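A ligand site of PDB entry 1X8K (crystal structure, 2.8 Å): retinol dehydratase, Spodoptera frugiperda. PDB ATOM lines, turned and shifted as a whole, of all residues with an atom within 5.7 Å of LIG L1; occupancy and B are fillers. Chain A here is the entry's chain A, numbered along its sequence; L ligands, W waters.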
ATOM      1  N   SER A  70      -2.775 -26.981  -0.886  1.00  0.00           N
ATOM      2  CA  SER A  70      -2.562 -26.148  -2.052  1.00  0.00           C
ATOM      3  C   SER A  70      -1.134 -26.310  -2.522  1.00  0.00           C
ATOM      4  O   SER A  70      -0.234 -26.553  -1.703  1.00  0.00           O
ATOM      5  CB  SER A  70      -2.791 -24.687  -1.661  1.00  0.00           C
ATOM      6  OG  SER A  70      -1.872 -24.319  -0.624  1.00  0.00           O
ATOM      7  N   TYR A  71      -0.905 -26.170  -3.823  1.00  0.00           N
ATOM      8  CA  TYR A  71       0.433 -25.748  -4.215  1.00  0.00           C
ATOM      9  C   TYR A  71       0.568 -24.332  -3.606  1.00  0.00           C
ATOM     10  O   TYR A  71      -0.430 -23.606  -3.512  1.00  0.00           O
ATOM     11  CB  TYR A  71       0.642 -25.755  -5.725  1.00  0.00           C
ATOM     12  CG  TYR A  71       2.059 -25.419  -6.048  1.00  0.00           C
ATOM     13  CD1 TYR A  71       3.041 -26.420  -6.083  1.00  0.00           C
ATOM     14  CD2 TYR A  71       2.457 -24.097  -6.191  1.00  0.00           C
ATOM     15  CE1 TYR A  71       4.387 -26.104  -6.314  1.00  0.00           C
ATOM     16  CE2 TYR A  71       3.778 -23.767  -6.424  1.00  0.00           C
ATOM     17  CZ  TYR A  71       4.728 -24.776  -6.485  1.00  0.00           C
ATOM     18  OH  TYR A  71       6.018 -24.413  -6.698  1.00  0.00           O
ATOM     19  N   GLN A  72       1.757 -23.964  -3.136  1.00  0.00           N
ATOM     20  CA  GLN A  72       1.928 -22.645  -2.496  1.00  0.00           C
ATOM     21  C   GLN A  72       1.443 -21.468  -3.354  1.00  0.00           C
ATOM     22  O   GLN A  72       1.386 -21.579  -4.562  1.00  0.00           O
ATOM     23  CB  GLN A  72       3.389 -22.418  -2.147  1.00  0.00           C
ATOM     24  CG  GLN A  72       4.267 -21.975  -3.334  1.00  0.00           C
ATOM     25  CD  GLN A  72       5.682 -21.655  -2.887  1.00  0.00           C
ATOM     26  OE1 GLN A  72       6.221 -20.606  -3.239  1.00  0.00           O
ATOM     27  NE2 GLN A  72       6.261 -22.537  -2.088  1.00  0.00           N
ATOM     28  N   ARG A  73       1.087 -20.367  -2.691  1.00  0.00           N
ATOM     29  CA  ARG A  73       0.679 -19.079  -3.328  1.00  0.00           C
ATOM     30  C   ARG A  73      -0.596 -19.135  -4.149  1.00  0.00           C
ATOM     31  O   ARG A  73      -0.774 -18.341  -5.087  1.00  0.00           O
ATOM     32  CB  ARG A  73       1.829 -18.427  -4.102  1.00  0.00           C
ATOM     33  CG  ARG A  73       3.093 -18.253  -3.299  1.00  0.00           C
ATOM     34  CD  ARG A  73       2.891 -17.502  -2.025  1.00  0.00           C
ATOM     35  NE  ARG A  73       2.880 -16.066  -2.268  1.00  0.00           N
ATOM     36  CZ  ARG A  73       2.631 -15.146  -1.353  1.00  0.00           C
ATOM     37  NH1 ARG A  73       2.352 -15.498  -0.113  1.00  0.00           N
ATOM     38  NH2 ARG A  73       2.653 -13.855  -1.668  1.00  0.00           N
ATOM     39  N   SER A  74      -1.479 -20.077  -3.778  1.00  0.00           N
ATOM     40  CA  SER A  74      -2.763 -20.311  -4.448  1.00  0.00           C
ATOM     41  C   SER A  74      -3.986 -19.777  -3.679  1.00  0.00           C
ATOM     42  O   SER A  74      -5.078 -19.828  -4.214  1.00  0.00           O
ATOM     43  CB  SER A  74      -2.967 -21.812  -4.720  1.00  0.00           C
ATOM     44  OG  SER A  74      -1.824 -22.428  -5.272  1.00  0.00           O
ATOM     45  N   GLY A  75      -3.821 -19.296  -2.446  1.00  0.00           N
ATOM     46  CA  GLY A  75      -4.959 -18.849  -1.659  1.00  0.00           C
ATOM     47  C   GLY A  75      -5.125 -19.522  -0.300  1.00  0.00           C
ATOM     48  O   GLY A  75      -6.199 -19.484   0.320  1.00  0.00           O
ATOM     49  N   THR A  76      -4.036 -20.120   0.177  1.00  0.00           N
ATOM     50  CA  THR A  76      -3.990 -20.776   1.484  1.00  0.00           C
ATOM     51  C   THR A  76      -4.437 -19.849   2.601  1.00  0.00           C
ATOM     52  O   THR A  76      -5.402 -20.166   3.301  1.00  0.00           O
ATOM     53  CB  THR A  76      -2.567 -21.288   1.750  1.00  0.00           C
ATOM     54  OG1 THR A  76      -2.021 -21.794   0.527  1.00  0.00           O
ATOM     55  CG2 THR A  76      -2.560 -22.472   2.706  1.00  0.00           C
ATOM     56  N   THR A  77      -3.778 -18.687   2.723  1.00  0.00           N
ATOM     57  CA  THR A  77      -4.011 -17.714   3.804  1.00  0.00           C
ATOM     58  C   THR A  77      -5.464 -17.264   3.915  1.00  0.00           C
ATOM     59  O   THR A  77      -6.040 -17.316   5.005  1.00  0.00           O
ATOM     60  CB  THR A  77      -3.019 -16.532   3.689  1.00  0.00           C
ATOM     61  OG1 THR A  77      -1.709 -17.056   3.468  1.00  0.00           O
ATOM     62  CG2 THR A  77      -2.833 -15.839   5.029  1.00  0.00           C
ATOM     63  N   MET A  78      -6.056 -16.852   2.802  1.00  0.00           N
ATOM     64  CA  MET A  78      -7.498 -16.582   2.697  1.00  0.00           C
ATOM     65  C   MET A  78      -8.360 -17.719   3.250  1.00  0.00           C
ATOM     66  O   MET A  78      -9.231 -17.530   4.122  1.00  0.00           O
ATOM     67  CB  MET A  78      -7.904 -16.427   1.228  1.00  0.00           C
ATOM     68  CG  MET A  78      -7.157 -15.385   0.445  1.00  0.00           C
ATOM     69  SD  MET A  78      -7.837 -15.255  -1.208  1.00  0.00           S
ATOM     70  CE  MET A  78      -9.376 -14.409  -0.871  1.00  0.00           C
ATOM     71  N   GLN A  80      -7.540 -20.512   5.028  1.00  0.00           N
ATOM     72  CA  GLN A  80      -7.265 -20.669   6.447  1.00  0.00           C
ATOM     73  C   GLN A  80      -8.078 -19.725   7.329  1.00  0.00           C
ATOM     74  O   GLN A  80      -8.719 -20.139   8.306  1.00  0.00           O
ATOM     75  CB  GLN A  80      -5.796 -20.398   6.699  1.00  0.00           C
ATOM     76  CG  GLN A  80      -4.844 -21.451   6.249  1.00  0.00           C
ATOM     77  CD  GLN A  80      -3.438 -21.083   6.644  1.00  0.00           C
ATOM     78  OE1 GLN A  80      -3.090 -21.143   7.834  1.00  0.00           O
ATOM     79  NE2 GLN A  80      -2.630 -20.689   5.674  1.00  0.00           N
ATOM     80  N   HIS A 164       1.559 -27.657   2.102  1.00  0.00           N
ATOM     81  CA  HIS A 164       1.765 -27.546   0.666  1.00  0.00           C
ATOM     82  C   HIS A 164       2.170 -28.913   0.105  1.00  0.00           C
ATOM     83  O   HIS A 164       2.632 -29.036  -1.036  1.00  0.00           O
ATOM     84  CB  HIS A 164       2.796 -26.453   0.397  1.00  0.00           C
ATOM     85  CG  HIS A 164       2.322 -25.068   0.724  1.00  0.00           C
ATOM     86  ND1 HIS A 164       1.193 -24.497   0.171  1.00  0.00           N
ATOM     87  CD2 HIS A 164       2.844 -24.126   1.559  1.00  0.00           C
ATOM     88  CE1 HIS A 164       1.034 -23.278   0.650  1.00  0.00           C
ATOM     89  NE2 HIS A 164       2.018 -23.022   1.491  1.00  0.00           N
ATOM     90  N   ARG A 185      -4.831 -22.545  -8.625  1.00  0.00           N
ATOM     91  CA  ARG A 185      -4.668 -21.200  -9.188  1.00  0.00           C
ATOM     92  C   ARG A 185      -3.876 -21.245 -10.497  1.00  0.00           C
ATOM     93  O   ARG A 185      -2.966 -22.063 -10.637  1.00  0.00           O
ATOM     94  CB  ARG A 185      -3.938 -20.322  -8.175  1.00  0.00           C
ATOM     95  CG  ARG A 185      -3.618 -18.944  -8.632  1.00  0.00           C
ATOM     96  CD  ARG A 185      -3.104 -18.086  -7.489  1.00  0.00           C
ATOM     97  NE  ARG A 185      -3.262 -16.670  -7.795  1.00  0.00           N
ATOM     98  CZ  ARG A 185      -2.478 -15.723  -7.340  1.00  0.00           C
ATOM     99  NH1 ARG A 185      -1.454 -16.025  -6.554  1.00  0.00           N
ATOM    100  NH2 ARG A 185      -2.714 -14.462  -7.693  1.00  0.00           N
ATOM    101  N   ASP A 189       0.183 -17.271 -12.660  1.00  0.00           N
ATOM    102  CA  ASP A 189       0.084 -16.334 -11.526  1.00  0.00           C
ATOM    103  C   ASP A 189       0.777 -16.883 -10.299  1.00  0.00           C
ATOM    104  O   ASP A 189       1.377 -16.129  -9.560  1.00  0.00           O
ATOM    105  CB  ASP A 189      -1.368 -15.984 -11.195  1.00  0.00           C
ATOM    106  CG  ASP A 189      -1.939 -14.912 -12.116  1.00  0.00           C
ATOM    107  OD1 ASP A 189      -1.440 -13.747 -12.103  1.00  0.00           O
ATOM    108  OD2 ASP A 189      -2.911 -15.121 -12.876  1.00  0.00           O
ATOM    109  N   VAL A 192       4.441 -16.065 -10.702  1.00  0.00           N
ATOM    110  CA  VAL A 192       4.771 -14.711 -10.291  1.00  0.00           C
ATOM    111  C   VAL A 192       4.672 -14.531  -8.780  1.00  0.00           C
ATOM    112  O   VAL A 192       5.601 -14.020  -8.162  1.00  0.00           O
ATOM    113  CB  VAL A 192       3.895 -13.649 -10.977  1.00  0.00           C
ATOM    114  CG1 VAL A 192       4.169 -12.298 -10.382  1.00  0.00           C
ATOM    115  CG2 VAL A 192       4.147 -13.627 -12.490  1.00  0.00           C
ATOM    116  N   SER A 193       3.568 -14.960  -8.172  1.00  0.00           N
ATOM    117  CA  SER A 193       3.476 -14.846  -6.725  1.00  0.00           C
ATOM    118  C   SER A 193       4.653 -15.556  -6.052  1.00  0.00           C
ATOM    119  O   SER A 193       5.300 -14.966  -5.188  1.00  0.00           O
ATOM    120  CB  SER A 193       2.150 -15.351  -6.161  1.00  0.00           C
ATOM    121  OG  SER A 193       2.010 -14.912  -4.811  1.00  0.00           O
ATOM    122  N   TYR A 248      -8.488 -20.097  -6.725  1.00  0.00           N
ATOM    123  CA  TYR A 248      -8.186 -18.762  -6.227  1.00  0.00           C
ATOM    124  C   TYR A 248      -9.055 -17.756  -6.933  1.00  0.00           C
ATOM    125  O   TYR A 248      -9.644 -16.880  -6.303  1.00  0.00           O
ATOM    126  CB  TYR A 248      -6.721 -18.422  -6.455  1.00  0.00           C
ATOM    127  CG  TYR A 248      -6.410 -16.993  -6.093  1.00  0.00           C
ATOM    128  CD1 TYR A 248      -6.374 -16.574  -4.758  1.00  0.00           C
ATOM    129  CD2 TYR A 248      -6.169 -16.044  -7.089  1.00  0.00           C
ATOM    130  CE1 TYR A 248      -6.094 -15.249  -4.436  1.00  0.00           C
ATOM    131  CE2 TYR A 248      -5.898 -14.728  -6.774  1.00  0.00           C
ATOM    132  CZ  TYR A 248      -5.864 -14.338  -5.455  1.00  0.00           C
ATOM    133  OH  TYR A 248      -5.583 -13.024  -5.163  1.00  0.00           O
ATOM    134  N   LEU A 252     -11.995 -14.151  -6.181  1.00  0.00           N
ATOM    135  CA  LEU A 252     -12.066 -12.814  -6.768  1.00  0.00           C
ATOM    136  C   LEU A 252     -13.393 -12.564  -7.466  1.00  0.00           C
ATOM    137  O   LEU A 252     -13.988 -11.490  -7.327  1.00  0.00           O
ATOM    138  CB  LEU A 252     -10.928 -12.572  -7.737  1.00  0.00           C
ATOM    139  CG  LEU A 252      -9.494 -12.618  -7.193  1.00  0.00           C
ATOM    140  CD1 LEU A 252      -8.532 -12.431  -8.317  1.00  0.00           C
ATOM    141  CD2 LEU A 252      -9.216 -11.560  -6.135  1.00  0.00           C
ATOM    142  N   LEU A 282     -12.279 -10.254   4.388  1.00  0.00           N
ATOM    143  CA  LEU A 282     -11.267 -10.742   3.455  1.00  0.00           C
ATOM    144  C   LEU A 282     -11.005  -9.764   2.338  1.00  0.00           C
ATOM    145  O   LEU A 282     -10.255 -10.078   1.412  1.00  0.00           O
ATOM    146  CB  LEU A 282     -11.682 -12.082   2.862  1.00  0.00           C
ATOM    147  CG  LEU A 282     -11.127 -13.370   3.475  1.00  0.00           C
ATOM    148  CD1 LEU A 282      -9.604 -13.357   3.579  1.00  0.00           C
ATOM    149  CD2 LEU A 282     -11.776 -13.600   4.846  1.00  0.00           C
ATOM    150  N   ASN A 283     -11.620  -8.584   2.416  1.00  0.00           N
ATOM    151  CA  ASN A 283     -11.270  -7.457   1.557  1.00  0.00           C
ATOM    152  C   ASN A 283      -9.759  -7.355   1.512  1.00  0.00           C
ATOM    153  O   ASN A 283      -9.089  -7.430   2.542  1.00  0.00           O
ATOM    154  CB  ASN A 283     -11.883  -6.161   2.122  1.00  0.00           C
ATOM    155  CG  ASN A 283     -11.376  -4.894   1.427  1.00  0.00           C
ATOM    156  OD1 ASN A 283     -11.057  -3.903   2.082  1.00  0.00           O
ATOM    157  ND2 ASN A 283     -11.328  -4.910   0.100  1.00  0.00           N
ATOM    158  N   PHE A 284      -9.217  -7.197   0.319  1.00  0.00           N
ATOM    159  CA  PHE A 284      -7.764  -7.320   0.170  1.00  0.00           C
ATOM    160  C   PHE A 284      -6.965  -6.317   1.020  1.00  0.00           C
ATOM    161  O   PHE A 284      -6.008  -6.697   1.701  1.00  0.00           O
ATOM    162  CB  PHE A 284      -7.351  -7.263  -1.301  1.00  0.00           C
ATOM    163  CG  PHE A 284      -5.911  -7.548  -1.519  1.00  0.00           C
ATOM    164  CD1 PHE A 284      -5.425  -8.865  -1.435  1.00  0.00           C
ATOM    165  CD2 PHE A 284      -5.008  -6.510  -1.756  1.00  0.00           C
ATOM    166  CE1 PHE A 284      -4.092  -9.138  -1.618  1.00  0.00           C
ATOM    167  CE2 PHE A 284      -3.666  -6.779  -1.939  1.00  0.00           C
ATOM    168  CZ  PHE A 284      -3.201  -8.096  -1.860  1.00  0.00           C
ATOM    169  N   PHE A 287      -7.442  -7.157   4.944  1.00  0.00           N
ATOM    170  CA  PHE A 287      -6.616  -8.341   5.191  1.00  0.00           C
ATOM    171  C   PHE A 287      -5.097  -8.068   5.179  1.00  0.00           C
ATOM    172  O   PHE A 287      -4.391  -8.421   6.127  1.00  0.00           O
ATOM    173  CB  PHE A 287      -6.976  -9.400   4.157  1.00  0.00           C
ATOM    174  CG  PHE A 287      -6.754 -10.806   4.620  1.00  0.00           C
ATOM    175  CD1 PHE A 287      -7.479 -11.325   5.677  1.00  0.00           C
ATOM    176  CD2 PHE A 287      -5.851 -11.618   3.960  1.00  0.00           C
ATOM    177  CE1 PHE A 287      -7.278 -12.626   6.080  1.00  0.00           C
ATOM    178  CE2 PHE A 287      -5.650 -12.919   4.363  1.00  0.00           C
ATOM    179  CZ  PHE A 287      -6.357 -13.425   5.426  1.00  0.00           C
ATOM    180  N   PHE A 310       4.078 -10.540   2.261  1.00  0.00           N
ATOM    181  CA  PHE A 310       3.418 -11.840   2.171  1.00  0.00           C
ATOM    182  C   PHE A 310       2.069 -11.752   1.442  1.00  0.00           C
ATOM    183  O   PHE A 310       1.710 -12.655   0.684  1.00  0.00           O
ATOM    184  CB  PHE A 310       3.235 -12.492   3.548  1.00  0.00           C
ATOM    185  CG  PHE A 310       2.793 -13.925   3.487  1.00  0.00           C
ATOM    186  CD1 PHE A 310       3.660 -14.926   2.994  1.00  0.00           C
ATOM    187  CD2 PHE A 310       1.503 -14.296   3.899  1.00  0.00           C
ATOM    188  CE1 PHE A 310       3.247 -16.290   2.934  1.00  0.00           C
ATOM    189  CE2 PHE A 310       1.096 -15.649   3.833  1.00  0.00           C
ATOM    190  CZ  PHE A 310       1.970 -16.640   3.333  1.00  0.00           C
ATOM    191  N   ILE A 311       1.347 -10.655   1.668  1.00  0.00           N
ATOM    192  CA  ILE A 311       0.106 -10.347   0.979  1.00  0.00           C
ATOM    193  C   ILE A 311       0.417  -9.187   0.049  1.00  0.00           C
ATOM    194  O   ILE A 311       0.624  -8.050   0.493  1.00  0.00           O
ATOM    195  CB  ILE A 311      -1.021  -9.997   1.987  1.00  0.00           C
ATOM    196  CG1 ILE A 311      -1.552 -11.262   2.663  1.00  0.00           C
ATOM    197  CG2 ILE A 311      -2.188  -9.385   1.291  1.00  0.00           C
ATOM    198  CD1 ILE A 311      -1.838 -11.104   4.143  1.00  0.00           C
ATOM    199  N   ARG A 312       0.423  -9.475  -1.252  1.00  0.00           N
ATOM    200  CA  ARG A 312       1.002  -8.619  -2.280  1.00  0.00           C
ATOM    201  C   ARG A 312      -0.041  -7.769  -3.050  1.00  0.00           C
ATOM    202  O   ARG A 312      -0.462  -6.713  -2.568  1.00  0.00           O
ATOM    203  CB  ARG A 312       1.761  -9.518  -3.245  1.00  0.00           C
ATOM    204  CG  ARG A 312       3.007  -8.971  -3.817  1.00  0.00           C
ATOM    205  CD  ARG A 312       3.732 -10.011  -4.640  1.00  0.00           C
ATOM    206  NE  ARG A 312       2.874 -10.560  -5.690  1.00  0.00           N
ATOM    207  CZ  ARG A 312       2.828 -10.105  -6.942  1.00  0.00           C
ATOM    208  NH1 ARG A 312       3.613  -9.103  -7.339  1.00  0.00           N
ATOM    209  NH2 ARG A 312       1.993 -10.670  -7.796  1.00  0.00           N
ATOM    210  N   LYS A 313      -0.430  -8.234  -4.233  1.00  0.00           N
ATOM    211  CA  LYS A 313      -1.379  -7.493  -5.080  1.00  0.00           C
ATOM    212  C   LYS A 313      -2.807  -8.023  -5.056  1.00  0.00           C
ATOM    213  O   LYS A 313      -3.747  -7.240  -5.150  1.00  0.00           O
ATOM    214  CB  LYS A 313      -0.876  -7.410  -6.516  1.00  0.00           C
ATOM    215  CG  LYS A 313      -0.178  -6.103  -6.823  1.00  0.00           C
ATOM    216  CD  LYS A 313      -0.694  -5.501  -8.122  1.00  0.00           C
ATOM    217  CE  LYS A 313      -0.131  -4.075  -8.290  1.00  0.00           C
ATOM    218  NZ  LYS A 313      -1.060  -3.227  -9.101  1.00  0.00           N
ATOM    219  N   GLY A 314      -2.966  -9.343  -4.948  1.00  0.00           N
ATOM    220  CA  GLY A 314      -4.261  -9.983  -4.813  1.00  0.00           C
ATOM    221  C   GLY A 314      -5.158  -9.911  -6.025  1.00  0.00           C
ATOM    222  O   GLY A 314      -6.383  -9.867  -5.887  1.00  0.00           O
ATOM    223  N   LYS A 315      -4.557  -9.898  -7.221  1.00  0.00           N
ATOM    224  CA  LYS A 315      -5.305  -9.928  -8.479  1.00  0.00           C
ATOM    225  C   LYS A 315      -5.015 -11.188  -9.312  1.00  0.00           C
ATOM    226  O   LYS A 315      -4.049 -11.884  -9.050  1.00  0.00           O
ATOM    227  CB  LYS A 315      -5.042  -8.672  -9.339  1.00  0.00           C
ATOM    228  CG  LYS A 315      -5.020  -7.350  -8.574  1.00  0.00           C
ATOM    229  CD  LYS A 315      -6.170  -6.412  -8.996  1.00  0.00           C
ATOM    230  CE  LYS A 315      -6.889  -5.801  -7.758  1.00  0.00           C
ATOM    231  NZ  LYS A 315      -7.723  -4.586  -8.095  1.00  0.00           N
HETATM  232  P1  LIG L   1      -0.289 -12.433  -5.086  1.00  0.00           P
HETATM  233  O1  LIG L   1      -0.665 -12.924  -6.466  1.00  0.00           O
HETATM  234  O2  LIG L   1      -0.860 -11.073  -4.756  1.00  0.00           O
HETATM  235  O3  LIG L   1       1.180 -12.586  -4.811  1.00  0.00           O
HETATM  236  P2  LIG L   1      -1.066 -18.193  -0.351  1.00  0.00           P
HETATM  237  O4  LIG L   1       0.425 -17.965  -0.370  1.00  0.00           O
HETATM  238  O5  LIG L   1      -1.729 -17.819   0.955  1.00  0.00           O
HETATM  239  O6  LIG L   1      -1.500 -19.553  -0.879  1.00  0.00           O
HETATM  240  O7  LIG L   1      -1.622 -17.107  -1.408  1.00  0.00           O
HETATM  241  C1  LIG L   1      -0.963 -15.861  -1.558  1.00  0.00           C
HETATM  242  C2  LIG L   1      -1.604 -15.032  -2.661  1.00  0.00           C
HETATM  243  O8  LIG L   1      -2.946 -14.741  -2.276  1.00  0.00           O
HETATM  244  C3  LIG L   1      -0.846 -13.716  -2.731  1.00  0.00           C
HETATM  245  O9  LIG L   1      -1.025 -13.498  -4.142  1.00  0.00           O
HETATM  246  C4  LIG L   1      -1.726 -12.675  -2.105  1.00  0.00           C
HETATM  247  O10 LIG L   1      -1.566 -11.318  -2.524  1.00  0.00           O
HETATM  248  C5  LIG L   1      -3.102 -13.324  -2.068  1.00  0.00           C
HETATM  249  N1  LIG L   1      -4.032 -12.914  -1.007  1.00  0.00           N
HETATM  250  C6  LIG L   1      -3.836 -12.959   0.323  1.00  0.00           C
HETATM  251  N2  LIG L   1      -4.940 -12.516   0.992  1.00  0.00           N
HETATM  252  C7  LIG L   1      -5.843 -12.206   0.043  1.00  0.00           C
HETATM  253  C8  LIG L   1      -7.151 -11.715   0.033  1.00  0.00           C
HETATM  254  N3  LIG L   1      -7.747 -11.440   1.223  1.00  0.00           N
HETATM  255  N4  LIG L   1      -7.803 -11.518  -1.155  1.00  0.00           N
HETATM  256  C9  LIG L   1      -7.210 -11.785  -2.351  1.00  0.00           C
HETATM  257  N5  LIG L   1      -5.944 -12.266  -2.420  1.00  0.00           N
HETATM  258  C10 LIG L   1      -5.255 -12.466  -1.174  1.00  0.00           C
HETATM  259  C1  LG2 L   2       3.536 -20.358   2.339  1.00  0.00           C
HETATM  260  C2  LG2 L   2       4.737 -19.833   2.727  1.00  0.00           C
HETATM  261  C3  LG2 L   2       5.224 -19.307   3.933  1.00  0.00           C
HETATM  262  C4  LG2 L   2       4.303 -18.808   5.092  1.00  0.00           C
HETATM  263  C5  LG2 L   2       6.606 -19.237   4.107  1.00  0.00           C
HETATM  264  C6  LG2 L   2       7.382 -18.784   5.167  1.00  0.00           C
HETATM  265  C7  LG2 L   2       8.283 -19.592   5.813  1.00  0.00           C
HETATM  266  C8  LG2 L   2       9.163 -19.472   6.870  1.00  0.00           C
HETATM  267  C9  LG2 L   2       8.695 -19.676   8.343  1.00  0.00           C
HETATM  268  C10 LG2 L   2      10.471 -19.189   6.556  1.00  0.00           C
HETATM  269  C11 LG2 L   2      11.533 -19.065   7.399  1.00  0.00           C
HETATM  270  C12 LG2 L   2      12.950 -18.970   7.457  1.00  0.00           C
HETATM  271  C13 LG2 L   2      14.070 -18.863   6.244  1.00  0.00           C
HETATM  272  C14 LG2 L   2      13.886 -17.577   5.381  1.00  0.00           C
HETATM  273  C15 LG2 L   2      14.229 -20.144   5.404  1.00  0.00           C
HETATM  274  C16 LG2 L   2      15.588 -18.738   6.606  1.00  0.00           C
HETATM  275  C17 LG2 L   2      15.950 -18.695   8.103  1.00  0.00           C
HETATM  276  C18 LG2 L   2      14.741 -18.800   9.041  1.00  0.00           C
HETATM  277  C19 LG2 L   2      13.410 -18.923   8.764  1.00  0.00           C
HETATM  278  C20 LG2 L   2      12.571 -18.986  10.084  1.00  0.00           C
HETATM  279  O   HOH W   1      -4.019 -16.400   0.460  1.00  0.00           O
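The side-chain hydroxyl of Ser 193 sits at hydrogen-bond distance from an oxygen (O3) of LIG L1 (2.5 Å).
O5 of LIG L1 sits at hydrogen-bond distance from N of Thr 77.
An oxygen (O5) of LIG L1 sits at hydrogen-bond distance from the side-chain hydroxyl (OG1) of Thr 77 (2.6 Å).
The backbone NH (N) of Thr 76 lies within hydrogen-bond range of an oxygen (O6) of LIG L1.
O6 of LIG L1 is in hydrogen-bond range of OG1 of Thr 76, 2.7 Å away.
O2 of LIG L1 is in hydrogen-bond range of N of Gly 314, at 2.7 Å.
N of Arg 312 lies within hydrogen-bond range of O10 of LIG L1 (3.0 Å).
O3 of LIG L1 lies within salt-bridge range of NE of Arg 312 (2.8 Å).
The backbone NH (N) of Gly 75 lies within hydrogen-bond range of an oxygen (O6) of LIG L1.
The guanidinium group (NH2) of Arg 185 lies within salt-bridge range of an oxygen (O1) of LIG L1.
N3 of LIG L1 sits at hydrogen-bond distance from O of Leu 282 (2.9 Å).
A nitrogen (N5) of LIG L1 lies within hydrogen-bond range of the side-chain hydroxyl of Tyr 248 (2.9 Å).
An oxygen (O2) of LIG L1 lies within hydrogen-bond range of the backbone NH (N) of Lys 313 (2.9 Å).
An oxygen (O6) of LIG L1 sits at hydrogen-bond distance from the backbone NH of Ser 74 (2.9 Å).
N of Arg 73 lies within hydrogen-bond range of O6 of LIG L1 (3.3 Å).
The guanidinium group (NH1) of Arg 73 is in salt-bridge range of an oxygen (O4) of LIG L1, 3.1 Å away.
The guanidinium group of Arg 73 is in hydrogen-bond range of the side-chain hydroxyl of Ser 193, 2.9 Å away.
OG1 of Thr 76 is in hydrogen-bond range of OG of Ser 70, at 2.8 Å.
The backbone carbonyl oxygen of Gly 314 sits close to the side-chain hydroxyl of Tyr 248 (3.3 Å).
The guanidinium group (NH1) of Arg 185 is in hydrogen-bond range of the backbone carbonyl oxygen (O) of Arg 73 (2.8 Å).
The guanidinium group (NH2) of Arg 185 is in hydrogen-bond range of the backbone carbonyl oxygen (O) of Lys 315 (3.2 Å).
OG of Ser 74 sits at hydrogen-bond distance from O of Gln 72, at 3.4 Å.
The backbone carbonyl oxygen (O) of Tyr 71 is in hydrogen-bond range of the side-chain hydroxyl (OG) of Ser 74 (2.5 Å).
The backbone carbonyl oxygen (O) of Phe 310 sits at hydrogen-bond distance from the guanidinium group (NH2) of Arg 73.
The side-chain sulfur (SD) of Met 78 lies close to a nitrogen (N4) of LIG L1, 3.7 Å away.
Merely in contact with LIG L1: Phe 287 (3.2 Å), Phe 284 (3.5 Å) and Ile 311 (3.7 Å).
Hydrophobic or aromatic side chains that line LIG L1: Met 78, Tyr 248, Leu 282, Phe 284, Phe 287 and Ile 311.
16 residues have an atom within 4 Å of LIG L1: Arg 73, Ser 74, Gly 75, Thr 76, Thr 77, Met 78, Arg 185, Ser 193, Tyr 248, Leu 282, Phe 284, Phe 287, Ile 311, Arg 312, Lys 313 and Gly 314.
Water W1 lies within hydrogen-bond range of O5 of LIG L1 (2.7 Å), N of Met 78 (3.1 Å) and N of Thr 77 (3.2 Å).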
